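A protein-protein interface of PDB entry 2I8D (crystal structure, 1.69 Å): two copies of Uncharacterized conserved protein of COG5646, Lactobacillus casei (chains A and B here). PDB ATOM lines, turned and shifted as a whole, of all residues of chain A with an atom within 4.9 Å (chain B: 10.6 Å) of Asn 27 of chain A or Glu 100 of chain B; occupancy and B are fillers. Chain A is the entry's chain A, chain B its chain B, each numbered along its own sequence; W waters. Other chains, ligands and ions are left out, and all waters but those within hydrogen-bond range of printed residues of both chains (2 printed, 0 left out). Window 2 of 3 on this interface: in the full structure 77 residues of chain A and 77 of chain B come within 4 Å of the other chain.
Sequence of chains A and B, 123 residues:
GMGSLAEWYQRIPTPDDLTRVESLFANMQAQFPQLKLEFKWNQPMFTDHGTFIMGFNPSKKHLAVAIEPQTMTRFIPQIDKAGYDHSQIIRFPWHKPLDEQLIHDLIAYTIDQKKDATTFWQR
Of the 9 printed residues of chain A, 4 touch a printed residue of chain B.
Hydrophobic or aromatic side chains of chain A that line the printed part of chain B: Leu 24 and Met 28.
Of the 17 printed residues of chain B, 4 touch a printed residue of chain A.
Hydrophobic or aromatic side chains of chain B within 4 Å of the printed part of chain A: Ile 103, His 104 and Ile 107.
Among the printed residues, 8 pairs touch across the chains.
Among the printed residues, merely in contact across the chains: Leu 24 of chain A with Glu 100 of chain B, Leu 24 of chain A with Ile 103 of chain B, Met 28 of chain A with Glu 100 of chain B, Met 28 of chain A with Ile 103 of chain B, Met 28 of chain A with His 104 of chain B and Met 28 of chain A with Ile 107 of chain B.
The side-chain carboxylate (OE1) of Glu 100 of chain B sits at hydrogen-bond distance from the side-chain amide nitrogen (ND2) of Asn 27 of chain A, at 2.9 Å.
The side-chain amide oxygen of Gln 31 of chain A is in hydrogen-bond range of a ring nitrogen (ND1) of His 104 of chain B (2.7 Å).
Asn 27 of chain A touches just one residue of chain B: Glu 100.
Of chain A, only Leu 24 (3.8 Å), Asn 27 (2.9 Å) and Met 28 (3.8 Å) come within 4 Å of Glu 100 of chain B.
No residue of chain B comes within 4 Å of Ser 23 of chain A.
No residue of chain B comes within 4 Å of Ala 26 of chain A.
Of chain B, only His 104 comes within 4 Å of Gln 31 of chain A.
Of the printed residues of chain B, Leu 24 of chain A touches Glu 100 and Ile 103.
Of the printed residues of chain A, Ile 107 of chain B touches Met 28 (3.8 Å).
Printed residues of chain A within 4 Å of Ile 103 of chain B: Leu 24 and Met 28.
Printed residues of chain A within 4 Å of His 104 of chain B: Met 28 (3.9 Å) and Gln 31 (2.7 Å).
The nearest residue of chain A that does not touch Glu 100 of chain B is Ser 23 of chain A (4.6 Å).
Water W2 lies within hydrogen-bond range of the side-chain carboxylate of Glu 100 of chain B (2.6 Å) and the side-chain amide nitrogen of Gln 31 of chain A (3.0 Å).
Water W1 bridges OE1 of Gln 101 of chain B and OE1 of Gln 31 of chain A.
The side-chain amide nitrogen of Asn 27 of chain A sits close to the backbone carbonyl oxygen of Ser 23 of chain A (3.3 Å).
No position is printed for both chains.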
ATOM      1  N   SER A  23     -30.273  -9.571   5.850  1.00  0.00           N
ATOM      2  CA  SER A  23     -29.889 -10.972   5.652  1.00  0.00           C
ATOM      3  C   SER A  23     -29.371 -11.612   6.926  1.00  0.00           C
ATOM      4  O   SER A  23     -29.690 -12.751   7.221  1.00  0.00           O
ATOM      5  CB  SER A  23     -28.797 -11.075   4.594  1.00  0.00           C
ATOM      6  OG  SER A  23     -29.321 -10.752   3.335  1.00  0.00           O
ATOM      7  N   LEU A  24     -28.543 -10.873   7.653  1.00  0.00           N
ATOM      8  CA  LEU A  24     -28.039 -11.348   8.927  1.00  0.00           C
ATOM      9  C   LEU A  24     -29.191 -11.664   9.858  1.00  0.00           C
ATOM     10  O   LEU A  24     -29.273 -12.756  10.423  1.00  0.00           O
ATOM     11  CB  LEU A  24     -27.122 -10.305   9.556  1.00  0.00           C
ATOM     12  CG  LEU A  24     -26.443 -10.725  10.872  1.00  0.00           C
ATOM     13  CD1 LEU A  24     -25.588 -11.980  10.712  1.00  0.00           C
ATOM     14  CD2 LEU A  24     -25.618  -9.543  11.372  1.00  0.00           C
ATOM     15  N   PHE A  25     -30.085 -10.703  10.033  1.00  0.00           N
ATOM     16  CA  PHE A  25     -31.212 -10.928  10.922  1.00  0.00           C
ATOM     17  C   PHE A  25     -32.035 -12.131  10.496  1.00  0.00           C
ATOM     18  O   PHE A  25     -32.359 -12.982  11.315  1.00  0.00           O
ATOM     19  CB  PHE A  25     -32.110  -9.690  10.983  1.00  0.00           C
ATOM     20  CG  PHE A  25     -31.498  -8.492  11.705  1.00  0.00           C
ATOM     21  CD1 PHE A  25     -30.272  -8.551  12.364  1.00  0.00           C
ATOM     22  CD2 PHE A  25     -32.201  -7.294  11.759  1.00  0.00           C
ATOM     23  CE1 PHE A  25     -29.769  -7.446  13.010  1.00  0.00           C
ATOM     24  CE2 PHE A  25     -31.687  -6.180  12.412  1.00  0.00           C
ATOM     25  CZ  PHE A  25     -30.499  -6.253  13.041  1.00  0.00           C
ATOM     26  N   ALA A  26     -32.356 -12.215   9.212  1.00  0.00           N
ATOM     27  CA  ALA A  26     -33.145 -13.340   8.695  1.00  0.00           C
ATOM     28  C   ALA A  26     -32.469 -14.675   8.901  1.00  0.00           C
ATOM     29  O   ALA A  26     -33.112 -15.632   9.341  1.00  0.00           O
ATOM     30  CB  ALA A  26     -33.444 -13.150   7.242  1.00  0.00           C
ATOM     31  N   ASN A  27     -31.179 -14.739   8.584  1.00  0.00           N
ATOM     32  CA  ASN A  27     -30.416 -15.975   8.749  1.00  0.00           C
ATOM     33  C   ASN A  27     -30.313 -16.382  10.216  1.00  0.00           C
ATOM     34  O   ASN A  27     -30.492 -17.548  10.554  1.00  0.00           O
ATOM     35  CB  ASN A  27     -29.008 -15.839   8.177  1.00  0.00           C
ATOM     36  CG  ASN A  27     -28.987 -15.687   6.664  1.00  0.00           C
ATOM     37  OD1 ASN A  27     -29.983 -15.948   5.975  1.00  0.00           O
ATOM     38  ND2 ASN A  27     -27.843 -15.277   6.141  1.00  0.00           N
ATOM     39  N   MET A  28     -30.043 -15.430  11.103  1.00  0.00           N
ATOM     40  CA  MET A  28     -29.930 -15.775  12.538  1.00  0.00           C
ATOM     41  C   MET A  28     -31.280 -16.246  13.118  1.00  0.00           C
ATOM     42  O   MET A  28     -31.317 -17.204  13.903  1.00  0.00           O
ATOM     43  CB  MET A  28     -29.353 -14.633  13.390  1.00  0.00           C
ATOM     44  CG  MET A  28     -27.872 -14.295  13.115  1.00  0.00           C
ATOM     45  SD  MET A  28     -26.615 -15.830  13.124  1.00  0.00           S
ATOM     46  CE  MET A  28     -26.475 -16.210  11.253  1.00  0.00           C
ATOM     47  N   GLN A  29     -32.375 -15.600  12.719  1.00  0.00           N
ATOM     48  CA  GLN A  29     -33.721 -16.033  13.136  1.00  0.00           C
ATOM     49  C   GLN A  29     -34.025 -17.444  12.618  1.00  0.00           C
ATOM     50  O   GLN A  29     -34.601 -18.277  13.332  1.00  0.00           O
ATOM     51  CB  GLN A  29     -34.791 -15.024  12.674  1.00  0.00           C
ATOM     52  CG  GLN A  29     -34.873 -13.738  13.533  1.00  0.00           C
ATOM     53  CD  GLN A  29     -35.586 -12.552  12.836  1.00  0.00           C
ATOM     54  OE1 GLN A  29     -35.248 -12.182  11.711  1.00  0.00           O
ATOM     55  NE2 GLN A  29     -36.554 -11.950  13.521  1.00  0.00           N
ATOM     56  N   ALA A  30     -33.597 -17.733  11.394  1.00  0.00           N
ATOM     57  CA  ALA A  30     -33.778 -19.075  10.832  1.00  0.00           C
ATOM     58  C   ALA A  30     -32.964 -20.105  11.620  1.00  0.00           C
ATOM     59  O   ALA A  30     -33.432 -21.217  11.881  1.00  0.00           O
ATOM     60  CB  ALA A  30     -33.424 -19.113   9.331  1.00  0.00           C
ATOM     61  N   GLN A  31     -31.765 -19.713  12.041  1.00  0.00           N
ATOM     62  CA  GLN A  31     -30.843 -20.629  12.735  1.00  0.00           C
ATOM     63  C   GLN A  31     -31.179 -20.825  14.200  1.00  0.00           C
ATOM     64  O   GLN A  31     -30.859 -21.882  14.781  1.00  0.00           O
ATOM     65  CB  GLN A  31     -29.405 -20.141  12.571  1.00  0.00           C
ATOM     66  CG  GLN A  31     -28.914 -20.384  11.157  1.00  0.00           C
ATOM     67  CD  GLN A  31     -27.658 -19.642  10.813  1.00  0.00           C
ATOM     68  OE1 GLN A  31     -26.810 -19.390  11.672  1.00  0.00           O
ATOM     69  NE2 GLN A  31     -27.554 -19.223   9.551  1.00  0.00           N
ATOM     70  N   ILE B  90     -18.070  -5.937  18.934  1.00  0.00           N
ATOM     71  CA  ILE B  90     -17.202  -6.302  17.838  1.00  0.00           C
ATOM     72  C   ILE B  90     -17.562  -5.420  16.660  1.00  0.00           C
ATOM     73  O   ILE B  90     -18.740  -5.282  16.323  1.00  0.00           O
ATOM     74  CB  ILE B  90     -17.383  -7.805  17.435  1.00  0.00           C
ATOM     75  CG1 ILE B  90     -17.159  -8.702  18.645  1.00  0.00           C
ATOM     76  CG2 ILE B  90     -16.439  -8.192  16.260  1.00  0.00           C
ATOM     77  CD1 ILE B  90     -17.511 -10.171  18.408  1.00  0.00           C
ATOM     78  N   PHE B  92     -17.683  -4.880  12.805  1.00  0.00           N
ATOM     79  CA  PHE B  92     -17.709  -5.581  11.546  1.00  0.00           C
ATOM     80  C   PHE B  92     -17.762  -4.487  10.462  1.00  0.00           C
ATOM     81  O   PHE B  92     -18.849  -3.915  10.167  1.00  0.00           O
ATOM     82  CB  PHE B  92     -18.913  -6.501  11.420  1.00  0.00           C
ATOM     83  CG  PHE B  92     -18.851  -7.706  12.298  1.00  0.00           C
ATOM     84  CD1 PHE B  92     -19.371  -7.696  13.592  1.00  0.00           C
ATOM     85  CD2 PHE B  92     -18.289  -8.860  11.823  1.00  0.00           C
ATOM     86  CE1 PHE B  92     -19.293  -8.829  14.385  1.00  0.00           C
ATOM     87  CE2 PHE B  92     -18.231  -9.988  12.602  1.00  0.00           C
ATOM     88  CZ  PHE B  92     -18.735  -9.969  13.889  1.00  0.00           C
ATOM     89  N   TRP B  94     -18.193  -2.304   7.208  1.00  0.00           N
ATOM     90  CA  TRP B  94     -19.093  -2.462   6.065  1.00  0.00           C
ATOM     91  C   TRP B  94     -18.360  -2.928   4.820  1.00  0.00           C
ATOM     92  O   TRP B  94     -18.929  -3.660   3.979  1.00  0.00           O
ATOM     93  CB  TRP B  94     -19.780  -1.146   5.747  1.00  0.00           C
ATOM     94  CG  TRP B  94     -20.698  -0.639   6.804  1.00  0.00           C
ATOM     95  CD1 TRP B  94     -20.612   0.540   7.435  1.00  0.00           C
ATOM     96  CD2 TRP B  94     -21.867  -1.294   7.314  1.00  0.00           C
ATOM     97  NE1 TRP B  94     -21.643   0.675   8.325  1.00  0.00           N
ATOM     98  CE2 TRP B  94     -22.429  -0.439   8.271  1.00  0.00           C
ATOM     99  CE3 TRP B  94     -22.477  -2.531   7.069  1.00  0.00           C
ATOM    100  CZ2 TRP B  94     -23.583  -0.761   8.970  1.00  0.00           C
ATOM    101  CZ3 TRP B  94     -23.633  -2.840   7.741  1.00  0.00           C
ATOM    102  CH2 TRP B  94     -24.168  -1.965   8.695  1.00  0.00           C
ATOM    103  N   LYS B  96     -15.698  -4.889   4.664  1.00  0.00           N
ATOM    104  CA  LYS B  96     -15.057  -6.213   4.846  1.00  0.00           C
ATOM    105  C   LYS B  96     -16.138  -7.291   4.929  1.00  0.00           C
ATOM    106  O   LYS B  96     -17.267  -7.004   5.332  1.00  0.00           O
ATOM    107  CB  LYS B  96     -14.227  -6.269   6.145  1.00  0.00           C
ATOM    108  CG  LYS B  96     -13.029  -5.356   6.188  1.00  0.00           C
ATOM    109  N   PRO B  97     -15.791  -8.549   4.602  1.00  0.00           N
ATOM    110  CA  PRO B  97     -16.759  -9.633   4.740  1.00  0.00           C
ATOM    111  C   PRO B  97     -17.273  -9.764   6.172  1.00  0.00           C
ATOM    112  O   PRO B  97     -16.532  -9.494   7.115  1.00  0.00           O
ATOM    113  CB  PRO B  97     -15.945 -10.868   4.343  1.00  0.00           C
ATOM    114  CG  PRO B  97     -14.901 -10.313   3.388  1.00  0.00           C
ATOM    115  CD  PRO B  97     -14.510  -9.035   4.057  1.00  0.00           C
ATOM    116  N   LEU B  98     -18.549 -10.128   6.303  1.00  0.00           N
ATOM    117  CA  LEU B  98     -19.183 -10.399   7.586  1.00  0.00           C
ATOM    118  C   LEU B  98     -19.214 -11.903   7.824  1.00  0.00           C
ATOM    119  O   LEU B  98     -19.871 -12.654   7.098  1.00  0.00           O
ATOM    120  CB  LEU B  98     -20.601  -9.847   7.577  1.00  0.00           C
ATOM    121  CG  LEU B  98     -21.454  -9.885   8.841  1.00  0.00           C
ATOM    122  CD1 LEU B  98     -21.238  -8.642   9.660  1.00  0.00           C
ATOM    123  CD2 LEU B  98     -22.948 -10.026   8.417  1.00  0.00           C
ATOM    124  N   ASP B  99     -18.494 -12.328   8.850  1.00  0.00           N
ATOM    125  CA  ASP B  99     -18.346 -13.731   9.193  1.00  0.00           C
ATOM    126  C   ASP B  99     -19.574 -14.200   9.989  1.00  0.00           C
ATOM    127  O   ASP B  99     -19.628 -14.039  11.214  1.00  0.00           O
ATOM    128  CB  ASP B  99     -17.065 -13.865  10.010  1.00  0.00           C
ATOM    129  CG  ASP B  99     -16.738 -15.297  10.413  1.00  0.00           C
ATOM    130  OD1 ASP B  99     -17.568 -16.200  10.225  1.00  0.00           O
ATOM    131  OD2 ASP B  99     -15.633 -15.487  10.949  1.00  0.00           O
ATOM    132  N   GLU B 100     -20.552 -14.775   9.289  1.00  0.00           N
ATOM    133  CA  GLU B 100     -21.801 -15.192   9.929  1.00  0.00           C
ATOM    134  C   GLU B 100     -21.608 -16.435  10.817  1.00  0.00           C
ATOM    135  O   GLU B 100     -22.340 -16.612  11.802  1.00  0.00           O
ATOM    136  CB  GLU B 100     -22.933 -15.380   8.910  1.00  0.00           C
ATOM    137  CG  GLU B 100     -23.321 -14.039   8.230  1.00  0.00           C
ATOM    138  CD  GLU B 100     -24.705 -14.032   7.577  1.00  0.00           C
ATOM    139  OE1 GLU B 100     -25.515 -14.963   7.828  1.00  0.00           O
ATOM    140  OE2 GLU B 100     -24.976 -13.076   6.794  1.00  0.00           O
ATOM    141  N   GLN B 101     -20.599 -17.252  10.526  1.00  0.00           N
ATOM    142  CA  GLN B 101     -20.277 -18.362  11.439  1.00  0.00           C
ATOM    143  C   GLN B 101     -19.868 -17.854  12.813  1.00  0.00           C
ATOM    144  O   GLN B 101     -20.265 -18.438  13.815  1.00  0.00           O
ATOM    145  CB  GLN B 101     -19.187 -19.285  10.885  1.00  0.00           C
ATOM    146  CG  GLN B 101     -19.057 -20.584  11.701  1.00  0.00           C
ATOM    147  CD  GLN B 101     -20.333 -21.449  11.671  1.00  0.00           C
ATOM    148  OE1 GLN B 101     -20.749 -21.892  10.600  1.00  0.00           O
ATOM    149  NE2 GLN B 101     -20.938 -21.706  12.848  1.00  0.00           N
ATOM    150  N   LEU B 102     -19.068 -16.776  12.857  1.00  0.00           N
ATOM    151  CA  LEU B 102     -18.670 -16.186  14.144  1.00  0.00           C
ATOM    152  C   LEU B 102     -19.896 -15.669  14.889  1.00  0.00           C
ATOM    153  O   LEU B 102     -20.031 -15.930  16.084  1.00  0.00           O
ATOM    154  CB  LEU B 102     -17.662 -15.055  13.956  1.00  0.00           C
ATOM    155  CG  LEU B 102     -17.168 -14.303  15.202  1.00  0.00           C
ATOM    156  CD1 LEU B 102     -16.528 -15.204  16.277  1.00  0.00           C
ATOM    157  CD2 LEU B 102     -16.177 -13.179  14.790  1.00  0.00           C
ATOM    158  N   ILE B 103     -20.774 -14.951  14.181  1.00  0.00           N
ATOM    159  CA  ILE B 103     -22.017 -14.429  14.795  1.00  0.00           C
ATOM    160  C   ILE B 103     -22.887 -15.620  15.294  1.00  0.00           C
ATOM    161  O   ILE B 103     -23.315 -15.631  16.451  1.00  0.00           O
ATOM    162  CB  ILE B 103     -22.797 -13.481  13.843  1.00  0.00           C
ATOM    163  CG1 ILE B 103     -21.952 -12.223  13.556  1.00  0.00           C
ATOM    164  CG2 ILE B 103     -24.109 -13.080  14.499  1.00  0.00           C
ATOM    165  CD1 ILE B 103     -22.402 -11.412  12.359  1.00  0.00           C
ATOM    166  N   HIS B 104     -23.075 -16.635  14.451  1.00  0.00           N
ATOM    167  CA  HIS B 104     -23.766 -17.865  14.880  1.00  0.00           C
ATOM    168  C   HIS B 104     -23.143 -18.438  16.179  1.00  0.00           C
ATOM    169  O   HIS B 104     -23.834 -18.732  17.164  1.00  0.00           O
ATOM    170  CB  HIS B 104     -23.734 -18.921  13.755  1.00  0.00           C
ATOM    171  CG  HIS B 104     -24.314 -20.240  14.138  1.00  0.00           C
ATOM    172  ND1 HIS B 104     -25.560 -20.651  13.723  1.00  0.00           N
ATOM    173  CD2 HIS B 104     -23.817 -21.250  14.904  1.00  0.00           C
ATOM    174  CE1 HIS B 104     -25.811 -21.853  14.218  1.00  0.00           C
ATOM    175  NE2 HIS B 104     -24.767 -22.239  14.934  1.00  0.00           N
ATOM    176  N   ASP B 105     -21.827 -18.643  16.182  1.00  0.00           N
ATOM    177  CA  ASP B 105     -21.180 -19.213  17.365  1.00  0.00           C
ATOM    178  C   ASP B 105     -21.348 -18.358  18.647  1.00  0.00           C
ATOM    179  O   ASP B 105     -21.556 -18.888  19.757  1.00  0.00           O
ATOM    180  CB  ASP B 105     -19.704 -19.412  17.090  1.00  0.00           C
ATOM    181  CG  ASP B 105     -19.429 -20.477  16.031  1.00  0.00           C
ATOM    182  OD1 ASP B 105     -20.332 -21.274  15.656  1.00  0.00           O
ATOM    183  OD2 ASP B 105     -18.274 -20.503  15.547  1.00  0.00           O
ATOM    184  N   LEU B 106     -21.252 -17.042  18.483  1.00  0.00           N
ATOM    185  CA  LEU B 106     -21.464 -16.097  19.589  1.00  0.00           C
ATOM    186  C   LEU B 106     -22.873 -16.229  20.180  1.00  0.00           C
ATOM    187  O   LEU B 106     -23.062 -16.246  21.407  1.00  0.00           O
ATOM    188  CB  LEU B 106     -21.178 -14.668  19.130  1.00  0.00           C
ATOM    189  CG  LEU B 106     -19.723 -14.242  18.871  1.00  0.00           C
ATOM    190  CD1 LEU B 106     -19.705 -12.930  18.022  1.00  0.00           C
ATOM    191  CD2 LEU B 106     -18.934 -14.060  20.170  1.00  0.00           C
ATOM    192  N   ILE B 107     -23.868 -16.314  19.306  1.00  0.00           N
ATOM    193  CA  ILE B 107     -25.247 -16.504  19.720  1.00  0.00           C
ATOM    194  C   ILE B 107     -25.429 -17.847  20.399  1.00  0.00           C
ATOM    195  O   ILE B 107     -26.013 -17.911  21.473  1.00  0.00           O
ATOM    196  CB  ILE B 107     -26.239 -16.397  18.532  1.00  0.00           C
ATOM    197  CG1 ILE B 107     -26.259 -14.978  18.002  1.00  0.00           C
ATOM    198  CG2 ILE B 107     -27.635 -16.916  18.922  1.00  0.00           C
ATOM    199  CD1 ILE B 107     -27.191 -14.779  16.772  1.00  0.00           C
ATOM    200  N   ALA B 108     -24.918 -18.918  19.793  1.00  0.00           N
ATOM    201  CA  ALA B 108     -25.111 -20.258  20.362  1.00  0.00           C
ATOM    202  C   ALA B 108     -24.528 -20.351  21.763  1.00  0.00           C
ATOM    203  O   ALA B 108     -25.140 -20.917  22.705  1.00  0.00           O
ATOM    204  CB  ALA B 108     -24.458 -21.277  19.464  1.00  0.00           C
ATOM    205  N   ILE B 111     -26.718 -18.273  24.209  1.00  0.00           N
ATOM    206  CA  ILE B 111     -27.952 -18.985  24.486  1.00  0.00           C
ATOM    207  C   ILE B 111     -27.714 -20.074  25.541  1.00  0.00           C
ATOM    208  O   ILE B 111     -28.447 -20.185  26.529  1.00  0.00           O
ATOM    209  CB  ILE B 111     -28.543 -19.593  23.203  1.00  0.00           C
ATOM    210  CG1 ILE B 111     -29.180 -18.473  22.363  1.00  0.00           C
ATOM    211  CG2 ILE B 111     -29.608 -20.652  23.485  1.00  0.00           C
ATOM    212  CD1 ILE B 111     -29.680 -18.951  20.999  1.00  0.00           C
HETATM  213  O   HOH W   1     -24.149 -21.308  10.519  1.00  0.00           O
HETATM  214  O   HOH W   2     -25.505 -17.531   8.087  1.00  0.00           O
